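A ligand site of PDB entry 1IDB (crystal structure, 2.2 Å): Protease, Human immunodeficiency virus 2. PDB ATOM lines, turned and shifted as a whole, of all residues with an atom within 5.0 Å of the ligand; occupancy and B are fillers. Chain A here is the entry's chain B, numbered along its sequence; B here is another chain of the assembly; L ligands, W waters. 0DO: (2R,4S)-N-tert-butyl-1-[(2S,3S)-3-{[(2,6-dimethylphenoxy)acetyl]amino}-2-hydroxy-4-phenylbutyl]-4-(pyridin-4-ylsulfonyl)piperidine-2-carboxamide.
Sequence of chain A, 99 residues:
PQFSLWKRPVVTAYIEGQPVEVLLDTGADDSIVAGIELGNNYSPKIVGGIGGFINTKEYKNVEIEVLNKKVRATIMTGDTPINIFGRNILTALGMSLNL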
ATOM      1  N   ARG A   8     -23.456  11.696  -7.138  1.00  0.00           N
ATOM      2  CA  ARG A   8     -22.543  10.561  -7.287  1.00  0.00           C
ATOM      3  C   ARG A   8     -22.143  10.123  -5.914  1.00  0.00           C
ATOM      4  O   ARG A   8     -21.840  10.946  -5.079  1.00  0.00           O
ATOM      5  CB  ARG A   8     -21.274  10.997  -8.002  1.00  0.00           C
ATOM      6  CG  ARG A   8     -21.514  11.571  -9.379  1.00  0.00           C
ATOM      7  CD  ARG A   8     -20.196  11.860 -10.052  1.00  0.00           C
ATOM      8  NE  ARG A   8     -20.331  12.109 -11.451  1.00  0.00           N
ATOM      9  CZ  ARG A   8     -19.353  12.597 -12.200  1.00  0.00           C
ATOM     10  NH1 ARG A   8     -18.181  12.918 -11.661  1.00  0.00           N
ATOM     11  NH2 ARG A   8     -19.536  12.771 -13.542  1.00  0.00           N
ATOM     12  N   LEU A  23     -15.442   7.142  -6.476  1.00  0.00           N
ATOM     13  CA  LEU A  23     -16.805   6.859  -6.852  1.00  0.00           C
ATOM     14  C   LEU A  23     -17.214   5.405  -6.538  1.00  0.00           C
ATOM     15  O   LEU A  23     -16.534   4.488  -6.905  1.00  0.00           O
ATOM     16  CB  LEU A  23     -16.883   7.128  -8.387  1.00  0.00           C
ATOM     17  CG  LEU A  23     -18.196   6.802  -9.029  1.00  0.00           C
ATOM     18  CD1 LEU A  23     -19.281   7.712  -8.451  1.00  0.00           C
ATOM     19  CD2 LEU A  23     -18.050   7.109 -10.495  1.00  0.00           C
ATOM     20  N   ASP A  25     -19.004   2.302  -7.440  1.00  0.00           N
ATOM     21  CA  ASP A  25     -19.561   1.955  -8.736  1.00  0.00           C
ATOM     22  C   ASP A  25     -19.964   0.519  -8.933  1.00  0.00           C
ATOM     23  O   ASP A  25     -19.179  -0.281  -9.343  1.00  0.00           O
ATOM     24  CB  ASP A  25     -18.477   2.358  -9.777  1.00  0.00           C
ATOM     25  CG  ASP A  25     -18.838   2.433 -11.209  1.00  0.00           C
ATOM     26  OD1 ASP A  25     -19.774   1.906 -11.710  1.00  0.00           O
ATOM     27  OD2 ASP A  25     -17.910   2.955 -11.929  1.00  0.00           O
ATOM     28  N   GLY A  27     -21.101  -0.705 -11.421  1.00  0.00           N
ATOM     29  CA  GLY A  27     -20.996  -1.023 -12.823  1.00  0.00           C
ATOM     30  C   GLY A  27     -19.588  -1.362 -13.245  1.00  0.00           C
ATOM     31  O   GLY A  27     -19.349  -1.797 -14.358  1.00  0.00           O
ATOM     32  N   ALA A  28     -18.655  -1.115 -12.341  1.00  0.00           N
ATOM     33  CA  ALA A  28     -17.260  -1.489 -12.496  1.00  0.00           C
ATOM     34  C   ALA A  28     -16.996  -2.801 -11.715  1.00  0.00           C
ATOM     35  O   ALA A  28     -17.339  -2.943 -10.523  1.00  0.00           O
ATOM     36  CB  ALA A  28     -16.414  -0.388 -11.902  1.00  0.00           C
ATOM     37  N   ASP A  29     -16.449  -3.803 -12.421  1.00  0.00           N
ATOM     38  CA  ASP A  29     -16.076  -5.097 -11.874  1.00  0.00           C
ATOM     39  C   ASP A  29     -14.884  -4.972 -10.941  1.00  0.00           C
ATOM     40  O   ASP A  29     -14.841  -5.572  -9.924  1.00  0.00           O
ATOM     41  CB  ASP A  29     -15.728  -6.053 -13.001  1.00  0.00           C
ATOM     42  CG  ASP A  29     -16.830  -6.420 -13.958  1.00  0.00           C
ATOM     43  OD1 ASP A  29     -18.027  -6.550 -13.451  1.00  0.00           O
ATOM     44  OD2 ASP A  29     -16.601  -6.854 -15.041  1.00  0.00           O
ATOM     45  N   ASP A  30     -13.907  -4.148 -11.311  1.00  0.00           N
ATOM     46  CA  ASP A  30     -12.686  -3.885 -10.577  1.00  0.00           C
ATOM     47  C   ASP A  30     -12.492  -2.401 -10.304  1.00  0.00           C
ATOM     48  O   ASP A  30     -13.432  -1.641 -10.495  1.00  0.00           O
ATOM     49  CB  ASP A  30     -11.389  -4.585 -11.111  1.00  0.00           C
ATOM     50  CG  ASP A  30     -11.512  -6.078 -11.387  1.00  0.00           C
ATOM     51  OD1 ASP A  30     -11.803  -6.860 -10.388  1.00  0.00           O
ATOM     52  OD2 ASP A  30     -11.423  -6.503 -12.493  1.00  0.00           O
ATOM     53  N   SER A  31     -11.348  -2.038  -9.726  1.00  0.00           N
ATOM     54  CA  SER A  31     -11.146  -0.717  -9.224  1.00  0.00           C
ATOM     55  C   SER A  31      -9.959  -0.032  -9.833  1.00  0.00           C
ATOM     56  O   SER A  31      -8.950  -0.652 -10.107  1.00  0.00           O
ATOM     57  CB  SER A  31     -10.984  -0.771  -7.707  1.00  0.00           C
ATOM     58  OG  SER A  31     -12.130  -1.337  -7.136  1.00  0.00           O
ATOM     59  N   ILE A  32     -10.084   1.248 -10.068  1.00  0.00           N
ATOM     60  CA  ILE A  32      -8.975   1.915 -10.689  1.00  0.00           C
ATOM     61  C   ILE A  32      -8.891   3.328 -10.219  1.00  0.00           C
ATOM     62  O   ILE A  32      -9.871   4.036 -10.254  1.00  0.00           O
ATOM     63  CB  ILE A  32      -8.972   1.797 -12.211  1.00  0.00           C
ATOM     64  CG1 ILE A  32      -7.911   2.704 -12.803  1.00  0.00           C
ATOM     65  CG2 ILE A  32     -10.326   2.225 -12.760  1.00  0.00           C
ATOM     66  CD1 ILE A  32      -7.903   2.584 -14.304  1.00  0.00           C
ATOM     67  N   VAL A  47      -8.020  -2.159 -19.394  1.00  0.00           N
ATOM     68  CA  VAL A  47      -9.418  -2.098 -18.940  1.00  0.00           C
ATOM     69  C   VAL A  47     -10.280  -1.413 -19.955  1.00  0.00           C
ATOM     70  O   VAL A  47      -9.914  -0.426 -20.515  1.00  0.00           O
ATOM     71  CB  VAL A  47      -9.684  -1.681 -17.473  1.00  0.00           C
ATOM     72  CG1 VAL A  47      -8.834  -0.472 -17.061  1.00  0.00           C
ATOM     73  CG2 VAL A  47     -11.147  -1.372 -17.253  1.00  0.00           C
ATOM     74  N   GLY A  48     -11.453  -1.908 -20.191  1.00  0.00           N
ATOM     75  CA  GLY A  48     -12.301  -1.246 -21.147  1.00  0.00           C
ATOM     76  C   GLY A  48     -13.564  -0.675 -20.557  1.00  0.00           C
ATOM     77  O   GLY A  48     -14.011  -1.047 -19.510  1.00  0.00           O
ATOM     78  N   GLY A  49     -14.118   0.286 -21.279  1.00  0.00           N
ATOM     79  CA  GLY A  49     -15.331   0.952 -20.907  1.00  0.00           C
ATOM     80  C   GLY A  49     -15.936   1.585 -22.138  1.00  0.00           C
ATOM     81  O   GLY A  49     -15.758   1.097 -23.252  1.00  0.00           O
ATOM     82  N   ILE A  50     -16.692   2.638 -21.905  1.00  0.00           N
ATOM     83  CA  ILE A  50     -17.355   3.338 -22.982  1.00  0.00           C
ATOM     84  C   ILE A  50     -16.240   4.062 -23.782  1.00  0.00           C
ATOM     85  O   ILE A  50     -15.314   4.632 -23.201  1.00  0.00           O
ATOM     86  CB  ILE A  50     -18.421   4.283 -22.340  1.00  0.00           C
ATOM     87  CG1 ILE A  50     -19.702   3.556 -21.913  1.00  0.00           C
ATOM     88  CG2 ILE A  50     -18.696   5.561 -23.113  1.00  0.00           C
ATOM     89  CD1 ILE A  50     -20.705   3.245 -23.043  1.00  0.00           C
ATOM     90  N   MET A  76      -6.039  -1.155  -9.593  1.00  0.00           N
ATOM     91  CA  MET A  76      -5.332  -0.842 -10.803  1.00  0.00           C
ATOM     92  C   MET A  76      -5.080   0.641 -10.774  1.00  0.00           C
ATOM     93  O   MET A  76      -5.848   1.332 -10.117  1.00  0.00           O
ATOM     94  CB  MET A  76      -6.131  -1.236 -12.063  1.00  0.00           C
ATOM     95  CG  MET A  76      -6.113  -2.724 -12.320  1.00  0.00           C
ATOM     96  SD  MET A  76      -7.128  -3.146 -13.723  1.00  0.00           S
ATOM     97  CE  MET A  76      -8.680  -2.879 -12.889  1.00  0.00           C
ATOM     98  N   THR A  80      -7.643   7.477 -15.485  1.00  0.00           N
ATOM     99  CA  THR A  80      -9.094   7.335 -15.397  1.00  0.00           C
ATOM    100  C   THR A  80      -9.609   8.703 -15.031  1.00  0.00           C
ATOM    101  O   THR A  80      -8.945   9.460 -14.309  1.00  0.00           O
ATOM    102  CB  THR A  80      -9.558   6.197 -14.454  1.00  0.00           C
ATOM    103  OG1 THR A  80     -10.935   6.320 -14.243  1.00  0.00           O
ATOM    104  CG2 THR A  80      -8.844   6.245 -13.121  1.00  0.00           C
ATOM    105  N   PRO A  81     -10.705   9.090 -15.634  1.00  0.00           N
ATOM    106  CA  PRO A  81     -11.195  10.439 -15.396  1.00  0.00           C
ATOM    107  C   PRO A  81     -11.607  10.695 -13.959  1.00  0.00           C
ATOM    108  O   PRO A  81     -11.350  11.745 -13.435  1.00  0.00           O
ATOM    109  CB  PRO A  81     -12.299  10.683 -16.428  1.00  0.00           C
ATOM    110  CG  PRO A  81     -12.193   9.562 -17.467  1.00  0.00           C
ATOM    111  CD  PRO A  81     -11.203   8.556 -16.950  1.00  0.00           C
ATOM    112  N   ILE A  82     -12.190   9.688 -13.307  1.00  0.00           N
ATOM    113  CA  ILE A  82     -12.638   9.674 -11.938  1.00  0.00           C
ATOM    114  C   ILE A  82     -12.058   8.392 -11.317  1.00  0.00           C
ATOM    115  O   ILE A  82     -11.807   7.437 -12.015  1.00  0.00           O
ATOM    116  CB  ILE A  82     -14.204   9.649 -11.982  1.00  0.00           C
ATOM    117  CG1 ILE A  82     -14.735  10.885 -12.711  1.00  0.00           C
ATOM    118  CG2 ILE A  82     -14.874   9.624 -10.605  1.00  0.00           C
ATOM    119  CD1 ILE A  82     -16.267  10.847 -12.967  1.00  0.00           C
ATOM    120  N   ILE A  84     -12.437   5.006  -9.550  1.00  0.00           N
ATOM    121  CA  ILE A  84     -13.534   4.080  -9.431  1.00  0.00           C
ATOM    122  C   ILE A  84     -13.224   2.972  -8.430  1.00  0.00           C
ATOM    123  O   ILE A  84     -12.150   2.398  -8.525  1.00  0.00           O
ATOM    124  CB  ILE A  84     -13.679   3.435 -10.807  1.00  0.00           C
ATOM    125  CG1 ILE A  84     -13.965   4.484 -11.885  1.00  0.00           C
ATOM    126  CG2 ILE A  84     -14.751   2.371 -10.848  1.00  0.00           C
ATOM    127  CD1 ILE A  84     -13.731   3.985 -13.313  1.00  0.00           C
ATOM    128  N   ARG B   8     -22.554  -9.066 -11.212  1.00  0.00           N
ATOM    129  CA  ARG B   8     -22.956  -7.768 -11.752  1.00  0.00           C
ATOM    130  C   ARG B   8     -24.428  -7.635 -11.509  1.00  0.00           C
ATOM    131  O   ARG B   8     -25.155  -8.594 -11.718  1.00  0.00           O
ATOM    132  CB  ARG B   8     -22.828  -7.872 -13.227  1.00  0.00           C
ATOM    133  CG  ARG B   8     -21.409  -7.748 -13.665  1.00  0.00           C
ATOM    134  CD  ARG B   8     -21.385  -7.334 -15.105  1.00  0.00           C
ATOM    135  NE  ARG B   8     -20.050  -6.955 -15.583  1.00  0.00           N
ATOM    136  CZ  ARG B   8     -19.654  -7.331 -16.804  1.00  0.00           C
ATOM    137  NH1 ARG B   8     -20.496  -8.051 -17.569  1.00  0.00           N
ATOM    138  NH2 ARG B   8     -18.418  -6.998 -17.246  1.00  0.00           N
ATOM    139  N   LEU B  23     -27.635  -3.182 -16.790  1.00  0.00           N
ATOM    140  CA  LEU B  23     -26.767  -3.193 -15.628  1.00  0.00           C
ATOM    141  C   LEU B  23     -27.150  -2.059 -14.736  1.00  0.00           C
ATOM    142  O   LEU B  23     -27.275  -0.983 -15.230  1.00  0.00           O
ATOM    143  CB  LEU B  23     -25.326  -3.006 -16.183  1.00  0.00           C
ATOM    144  CG  LEU B  23     -24.206  -2.855 -15.148  1.00  0.00           C
ATOM    145  CD1 LEU B  23     -24.107  -4.148 -14.331  1.00  0.00           C
ATOM    146  CD2 LEU B  23     -22.880  -2.635 -15.886  1.00  0.00           C
ATOM    147  N   ASP B  25     -26.045   0.692 -12.509  1.00  0.00           N
ATOM    148  CA  ASP B  25     -24.777   1.387 -12.370  1.00  0.00           C
ATOM    149  C   ASP B  25     -24.806   2.703 -11.604  1.00  0.00           C
ATOM    150  O   ASP B  25     -25.230   3.727 -12.136  1.00  0.00           O
ATOM    151  CB  ASP B  25     -24.296   1.637 -13.808  1.00  0.00           C
ATOM    152  CG  ASP B  25     -22.806   1.874 -14.000  1.00  0.00           C
ATOM    153  OD1 ASP B  25     -22.120   2.150 -12.935  1.00  0.00           O
ATOM    154  OD2 ASP B  25     -22.290   1.821 -15.078  1.00  0.00           O
ATOM    155  N   GLY B  27     -22.315   4.443 -10.911  1.00  0.00           N
ATOM    156  CA  GLY B  27     -21.253   5.319 -11.392  1.00  0.00           C
ATOM    157  C   GLY B  27     -21.547   5.966 -12.729  1.00  0.00           C
ATOM    158  O   GLY B  27     -20.784   6.788 -13.259  1.00  0.00           O
ATOM    159  N   ALA B  28     -22.686   5.598 -13.295  1.00  0.00           N
ATOM    160  CA  ALA B  28     -23.121   6.215 -14.521  1.00  0.00           C
ATOM    161  C   ALA B  28     -24.141   7.310 -14.172  1.00  0.00           C
ATOM    162  O   ALA B  28     -25.118   7.016 -13.494  1.00  0.00           O
ATOM    163  CB  ALA B  28     -23.695   5.102 -15.372  1.00  0.00           C
ATOM    164  N   ASP B  29     -23.913   8.565 -14.625  1.00  0.00           N
ATOM    165  CA  ASP B  29     -24.791   9.687 -14.397  1.00  0.00           C
ATOM    166  C   ASP B  29     -26.057   9.595 -15.199  1.00  0.00           C
ATOM    167  O   ASP B  29     -27.143   9.930 -14.722  1.00  0.00           O
ATOM    168  CB  ASP B  29     -24.092  11.004 -14.728  1.00  0.00           C
ATOM    169  CG  ASP B  29     -22.855  11.276 -13.923  1.00  0.00           C
ATOM    170  OD1 ASP B  29     -22.771  11.002 -12.759  1.00  0.00           O
ATOM    171  OD2 ASP B  29     -21.947  12.012 -14.555  1.00  0.00           O
ATOM    172  N   ASP B  30     -25.899   9.082 -16.422  1.00  0.00           N
ATOM    173  CA  ASP B  30     -26.963   8.886 -17.411  1.00  0.00           C
ATOM    174  C   ASP B  30     -27.137   7.441 -17.869  1.00  0.00           C
ATOM    175  O   ASP B  30     -26.450   6.549 -17.372  1.00  0.00           O
ATOM    176  CB  ASP B  30     -26.749   9.826 -18.601  1.00  0.00           C
ATOM    177  CG  ASP B  30     -26.666  11.282 -18.163  1.00  0.00           C
ATOM    178  OD1 ASP B  30     -27.449  11.841 -17.369  1.00  0.00           O
ATOM    179  OD2 ASP B  30     -25.647  11.898 -18.704  1.00  0.00           O
ATOM    180  N   ILE B  32     -27.660   4.428 -20.990  1.00  0.00           N
ATOM    181  CA  ILE B  32     -27.381   4.186 -22.368  1.00  0.00           C
ATOM    182  C   ILE B  32     -27.628   2.772 -22.704  1.00  0.00           C
ATOM    183  O   ILE B  32     -27.233   1.882 -21.970  1.00  0.00           O
ATOM    184  CB  ILE B  32     -26.044   4.735 -22.869  1.00  0.00           C
ATOM    185  CG1 ILE B  32     -25.724   4.399 -24.312  1.00  0.00           C
ATOM    186  CG2 ILE B  32     -24.880   4.395 -21.962  1.00  0.00           C
ATOM    187  CD1 ILE B  32     -24.623   5.325 -24.782  1.00  0.00           C
ATOM    188  N   VAL B  47     -20.827  11.406 -25.260  1.00  0.00           N
ATOM    189  CA  VAL B  47     -20.763  10.818 -23.924  1.00  0.00           C
ATOM    190  C   VAL B  47     -19.438  10.158 -23.731  1.00  0.00           C
ATOM    191  O   VAL B  47     -19.035   9.369 -24.606  1.00  0.00           O
ATOM    192  CB  VAL B  47     -21.909   9.835 -23.556  1.00  0.00           C
ATOM    193  CG1 VAL B  47     -22.095   9.795 -22.037  1.00  0.00           C
ATOM    194  CG2 VAL B  47     -23.252  10.203 -24.192  1.00  0.00           C
ATOM    195  N   GLY B  48     -18.843  10.544 -22.587  1.00  0.00           N
ATOM    196  CA  GLY B  48     -17.521  10.215 -22.066  1.00  0.00           C
ATOM    197  C   GLY B  48     -17.491   9.050 -21.090  1.00  0.00           C
ATOM    198  O   GLY B  48     -18.211   8.938 -20.109  1.00  0.00           O
ATOM    199  N   GLY B  49     -16.608   8.163 -21.398  1.00  0.00           N
ATOM    200  CA  GLY B  49     -16.418   7.028 -20.585  1.00  0.00           C
ATOM    201  C   GLY B  49     -14.948   6.881 -20.359  1.00  0.00           C
ATOM    202  O   GLY B  49     -14.179   7.784 -20.650  1.00  0.00           O
ATOM    203  N   ILE B  50     -14.575   5.707 -19.863  1.00  0.00           N
ATOM    204  CA  ILE B  50     -13.199   5.433 -19.570  1.00  0.00           C
ATOM    205  C   ILE B  50     -12.279   5.500 -20.763  1.00  0.00           C
ATOM    206  O   ILE B  50     -11.188   6.051 -20.599  1.00  0.00           O
ATOM    207  CB  ILE B  50     -12.982   4.195 -18.686  1.00  0.00           C
ATOM    208  CG1 ILE B  50     -12.136   4.585 -17.484  1.00  0.00           C
ATOM    209  CG2 ILE B  50     -12.307   3.068 -19.486  1.00  0.00           C
ATOM    210  CD1 ILE B  50     -12.376   3.714 -16.262  1.00  0.00           C
ATOM    211  N   PHE B  53     -14.800   9.076 -26.131  1.00  0.00           N
ATOM    212  CA  PHE B  53     -16.145   9.642 -26.270  1.00  0.00           C
ATOM    213  C   PHE B  53     -16.960   8.915 -27.259  1.00  0.00           C
ATOM    214  O   PHE B  53     -16.387   8.399 -28.203  1.00  0.00           O
ATOM    215  CB  PHE B  53     -16.113  11.106 -26.729  1.00  0.00           C
ATOM    216  CG  PHE B  53     -15.804  11.963 -25.550  1.00  0.00           C
ATOM    217  CD1 PHE B  53     -14.491  12.081 -25.093  1.00  0.00           C
ATOM    218  CD2 PHE B  53     -16.836  12.504 -24.781  1.00  0.00           C
ATOM    219  CE1 PHE B  53     -14.224  12.825 -23.941  1.00  0.00           C
ATOM    220  CE2 PHE B  53     -16.576  13.256 -23.631  1.00  0.00           C
ATOM    221  CZ  PHE B  53     -15.265  13.404 -23.202  1.00  0.00           C
ATOM    222  N   PRO B  81     -21.268  -1.558 -25.137  1.00  0.00           N
ATOM    223  CA  PRO B  81     -21.078  -2.960 -24.948  1.00  0.00           C
ATOM    224  C   PRO B  81     -22.062  -3.564 -23.994  1.00  0.00           C
ATOM    225  O   PRO B  81     -22.435  -4.725 -24.135  1.00  0.00           O
ATOM    226  CB  PRO B  81     -19.705  -3.135 -24.380  1.00  0.00           C
ATOM    227  CG  PRO B  81     -19.099  -1.759 -24.194  1.00  0.00           C
ATOM    228  CD  PRO B  81     -20.123  -0.747 -24.643  1.00  0.00           C
ATOM    229  N   ILE B  82     -22.470  -2.777 -22.983  1.00  0.00           N
ATOM    230  CA  ILE B  82     -23.455  -3.247 -21.991  1.00  0.00           C
ATOM    231  C   ILE B  82     -24.568  -2.215 -21.840  1.00  0.00           C
ATOM    232  O   ILE B  82     -24.276  -1.043 -21.749  1.00  0.00           O
ATOM    233  CB  ILE B  82     -22.766  -3.483 -20.628  1.00  0.00           C
ATOM    234  CG1 ILE B  82     -21.605  -4.427 -20.757  1.00  0.00           C
ATOM    235  CG2 ILE B  82     -23.688  -4.086 -19.586  1.00  0.00           C
ATOM    236  CD1 ILE B  82     -20.893  -4.584 -19.423  1.00  0.00           C
ATOM    237  N   ILE B  84     -26.772   0.084 -19.889  1.00  0.00           N
ATOM    238  CA  ILE B  84     -26.634   0.765 -18.637  1.00  0.00           C
ATOM    239  C   ILE B  84     -27.818   1.597 -18.201  1.00  0.00           C
ATOM    240  O   ILE B  84     -28.288   2.436 -18.938  1.00  0.00           O
ATOM    241  CB  ILE B  84     -25.362   1.592 -18.728  1.00  0.00           C
ATOM    242  CG1 ILE B  84     -24.159   0.655 -18.607  1.00  0.00           C
ATOM    243  CG2 ILE B  84     -25.302   2.669 -17.676  1.00  0.00           C
ATOM    244  CD1 ILE B  84     -22.944   1.151 -19.372  1.00  0.00           C
HETATM  245  C1  0DO L   1     -16.264   1.211 -16.838  1.00  0.00           C
HETATM  246  C2  0DO L   1     -15.058   0.331 -16.545  1.00  0.00           C
HETATM  247  C1' 0DO L   1     -14.711  -1.628 -15.301  1.00  0.00           C
HETATM  248  C2' 0DO L   1     -15.229  -2.858 -15.776  1.00  0.00           C
HETATM  249  C3' 0DO L   1     -14.545  -4.053 -15.584  1.00  0.00           C
HETATM  250  C4' 0DO L   1     -13.342  -4.059 -14.876  1.00  0.00           C
HETATM  251  C5' 0DO L   1     -12.867  -2.847 -14.346  1.00  0.00           C
HETATM  252  C6' 0DO L   1     -13.527  -1.636 -14.551  1.00  0.00           C
HETATM  253  CM2 0DO L   1     -16.506  -2.941 -16.519  1.00  0.00           C
HETATM  254  CM6 0DO L   1     -12.985  -0.337 -13.967  1.00  0.00           C
HETATM  255  O1  0DO L   1     -16.149   2.127 -17.666  1.00  0.00           O
HETATM  256  O1' 0DO L   1     -15.378  -0.488 -15.415  1.00  0.00           O
HETATM  257  N   0DO L   1     -17.409   0.968 -16.143  1.00  0.00           N
HETATM  258  CA  0DO L   1     -18.553   1.838 -16.418  1.00  0.00           C
HETATM  259  C   0DO L   1     -18.867   2.646 -15.169  1.00  0.00           C
HETATM  260  OXT 0DO L   1     -19.632   1.908 -14.247  1.00  0.00           O
HETATM  261  CB  0DO L   1     -19.700   1.023 -17.046  1.00  0.00           C
HETATM  262  CG  0DO L   1     -19.314   0.224 -18.293  1.00  0.00           C
HETATM  263  CD1 0DO L   1     -19.322   0.783 -19.576  1.00  0.00           C
HETATM  264  CD2 0DO L   1     -18.946  -1.126 -18.208  1.00  0.00           C
HETATM  265  CE1 0DO L   1     -18.979   0.026 -20.702  1.00  0.00           C
HETATM  266  CE2 0DO L   1     -18.628  -1.899 -19.321  1.00  0.00           C
HETATM  267  CZ  0DO L   1     -18.606  -1.311 -20.589  1.00  0.00           C
HETATM  268  CM  0DO L   1     -19.588   3.973 -15.314  1.00  0.00           C
HETATM  269  N1  0DO L   1     -18.574   4.893 -15.696  1.00  0.00           N
HETATM  270  C21 0DO L   1     -19.023   6.021 -16.558  1.00  0.00           C
HETATM  271  C3  0DO L   1     -17.853   6.933 -16.792  1.00  0.00           C
HETATM  272  C4  0DO L   1     -16.999   7.213 -15.612  1.00  0.00           C
HETATM  273  C5  0DO L   1     -16.509   5.949 -15.075  1.00  0.00           C
HETATM  274  C6  0DO L   1     -17.779   5.307 -14.535  1.00  0.00           C
HETATM  275  C7  0DO L   1     -19.676   5.692 -17.876  1.00  0.00           C
HETATM  276  O   0DO L   1     -19.037   4.973 -18.700  1.00  0.00           O
HETATM  277  N11 0DO L   1     -16.886  12.082 -18.298  1.00  0.00           N
HETATM  278  C22 0DO L   1     -17.497  11.754 -17.140  1.00  0.00           C
HETATM  279  C31 0DO L   1     -17.141  10.564 -16.476  1.00  0.00           C
HETATM  280  C41 0DO L   1     -16.174   9.744 -17.013  1.00  0.00           C
HETATM  281  C51 0DO L   1     -15.570  10.122 -18.206  1.00  0.00           C
HETATM  282  C61 0DO L   1     -15.944  11.309 -18.829  1.00  0.00           C
HETATM  283  S   0DO L   1     -15.736   8.296 -16.235  1.00  0.00           S
HETATM  284  O1S 0DO L   1     -14.955   7.702 -17.258  1.00  0.00           O
HETATM  285  O2S 0DO L   1     -14.673   8.288 -15.329  1.00  0.00           O
HETATM  286  N2  0DO L   1     -20.889   6.361 -17.959  1.00  0.00           N
HETATM  287 C1'1 0DO L   1     -21.755   6.205 -19.058  1.00  0.00           C
HETATM  288 C2'1 0DO L   1     -23.044   7.045 -18.870  1.00  0.00           C
HETATM  289 C3'1 0DO L   1     -22.190   4.743 -19.168  1.00  0.00           C
HETATM  290 C4'1 0DO L   1     -21.059   6.646 -20.343  1.00  0.00           C
HETATM  291  O   HOH W   1     -16.632   4.094 -19.285  1.00  0.00           O
HETATM  292  O   HOH W   2     -21.137   8.757 -16.276  1.00  0.00           O
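An oxygen (OXT) of the ligand is in hydrogen-bond range of the side-chain carboxylate (OD1) of Asp 25 of chain A (2.5 Å).
An oxygen (OXT) of the ligand sits at hydrogen-bond distance from the side-chain carboxylate of Asp 25 of chain B, 2.8 Å away.
The backbone NH (N) of Ile 50 of chain B sits at hydrogen-bond distance from an oxygen (O1S) of the ligand (3.3 Å).
The backbone NH (N) of Ile 82 of chain A sits at hydrogen-bond distance from an oxygen (O2S) of the ligand (3.5 Å).
The side-chain carboxylate (OD1) of Asp 25 of chain A lies close to the side-chain carboxylate (OD1) of Asp 25 of chain B (2.7 Å).
N of Ala 28 of chain A lies within hydrogen-bond range of OD1 of Asp 25 of chain A (3.3 Å).
The side-chain carboxylate (OD1) of Asp 25 of chain B lies close to the backbone NH (N) of Gly 27 of chain A (3.4 Å).
The side-chain carboxylate (OD1) of Asp 25 of chain B lies within hydrogen-bond range of the backbone NH (N) of Gly 27 of chain B (3.1 Å).
The side-chain carboxylate (OD2) of Asp 29 of chain A is in salt-bridge range of the guanidinium group (NH2) of Arg 8 of chain B (2.9 Å).
O of Ile 82 of chain A lies within hydrogen-bond range of OG1 of Thr 80.
The backbone NH (N) of Ile 84 of chain B lies within hydrogen-bond range of the backbone carbonyl oxygen (O) of Ile 32 of chain B, at 2.8 Å.
O of Ile 84 of chain A sits at hydrogen-bond distance from N of Ile 32 of chain A.
O of Gly 49 of chain B sits close to O1S of the ligand, 3.5 Å away.
Merely in contact with the ligand: Pro 81 of chain A, Gly 27 of chain A, Gly 48 of chain A, Asp 30 of chain A, Gly 48 of chain B, Asp 29 of chain A, Ile 82 of chain B, Gly 49 of chain A, Ile 50 of chain A, Gly 27 of chain B, Val 47 of chain A, Ala 28 of chain A, Ile 84 of chain B, Pro 81 of chain B, Val 47 of chain B, Asp 30 of chain B, Ile 84 of chain A, Ile 32 of chain A and Ile 32 of chain B.
Hydrophobic or aromatic side chains that line the ligand: Ala 28 of chain A, Ile 32 of chain A, Val 47 of chain A, Ile 50 of chain A, Pro 81 of chain A, Ile 82 of chain A, Ile 84 of chain A, Ile 32 of chain B, Val 47 of chain B, Ile 50 of chain B, Pro 81 of chain B, Ile 82 of chain B and Ile 84 of chain B.
Within 4 Å of the ligand: Asp 25 of chain A, Gly 27 of chain A, Ala 28 of chain A, Asp 29 of chain A, Asp 30 of chain A, Ile 32 of chain A, Val 47 of chain A, Gly 48 of chain A, Gly 49 of chain A, Ile 50 of chain A, Pro 81 of chain A, Ile 82 of chain A, Ile 84 of chain A, Asp 25 of chain B, Gly 27 of chain B, Asp 30 of chain B, Ile 32 of chain B, Val 47 of chain B, Gly 48 of chain B, Gly 49 of chain B, Ile 50 of chain B, Pro 81 of chain B, Ile 82 of chain B and Ile 84 of chain B.
The nearest printed residue that does not touch the ligand is Ala 28 of chain B (4.02 Å).
Water W1 lies within hydrogen-bond range of O1 of the ligand (2.6 Å), N of Ile 50 of chain B (2.7 Å) and N of Ile 50 of chain A (3.0 Å).
Water W2 bridges N2 of the ligand and N of Asp 29 of chain B.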
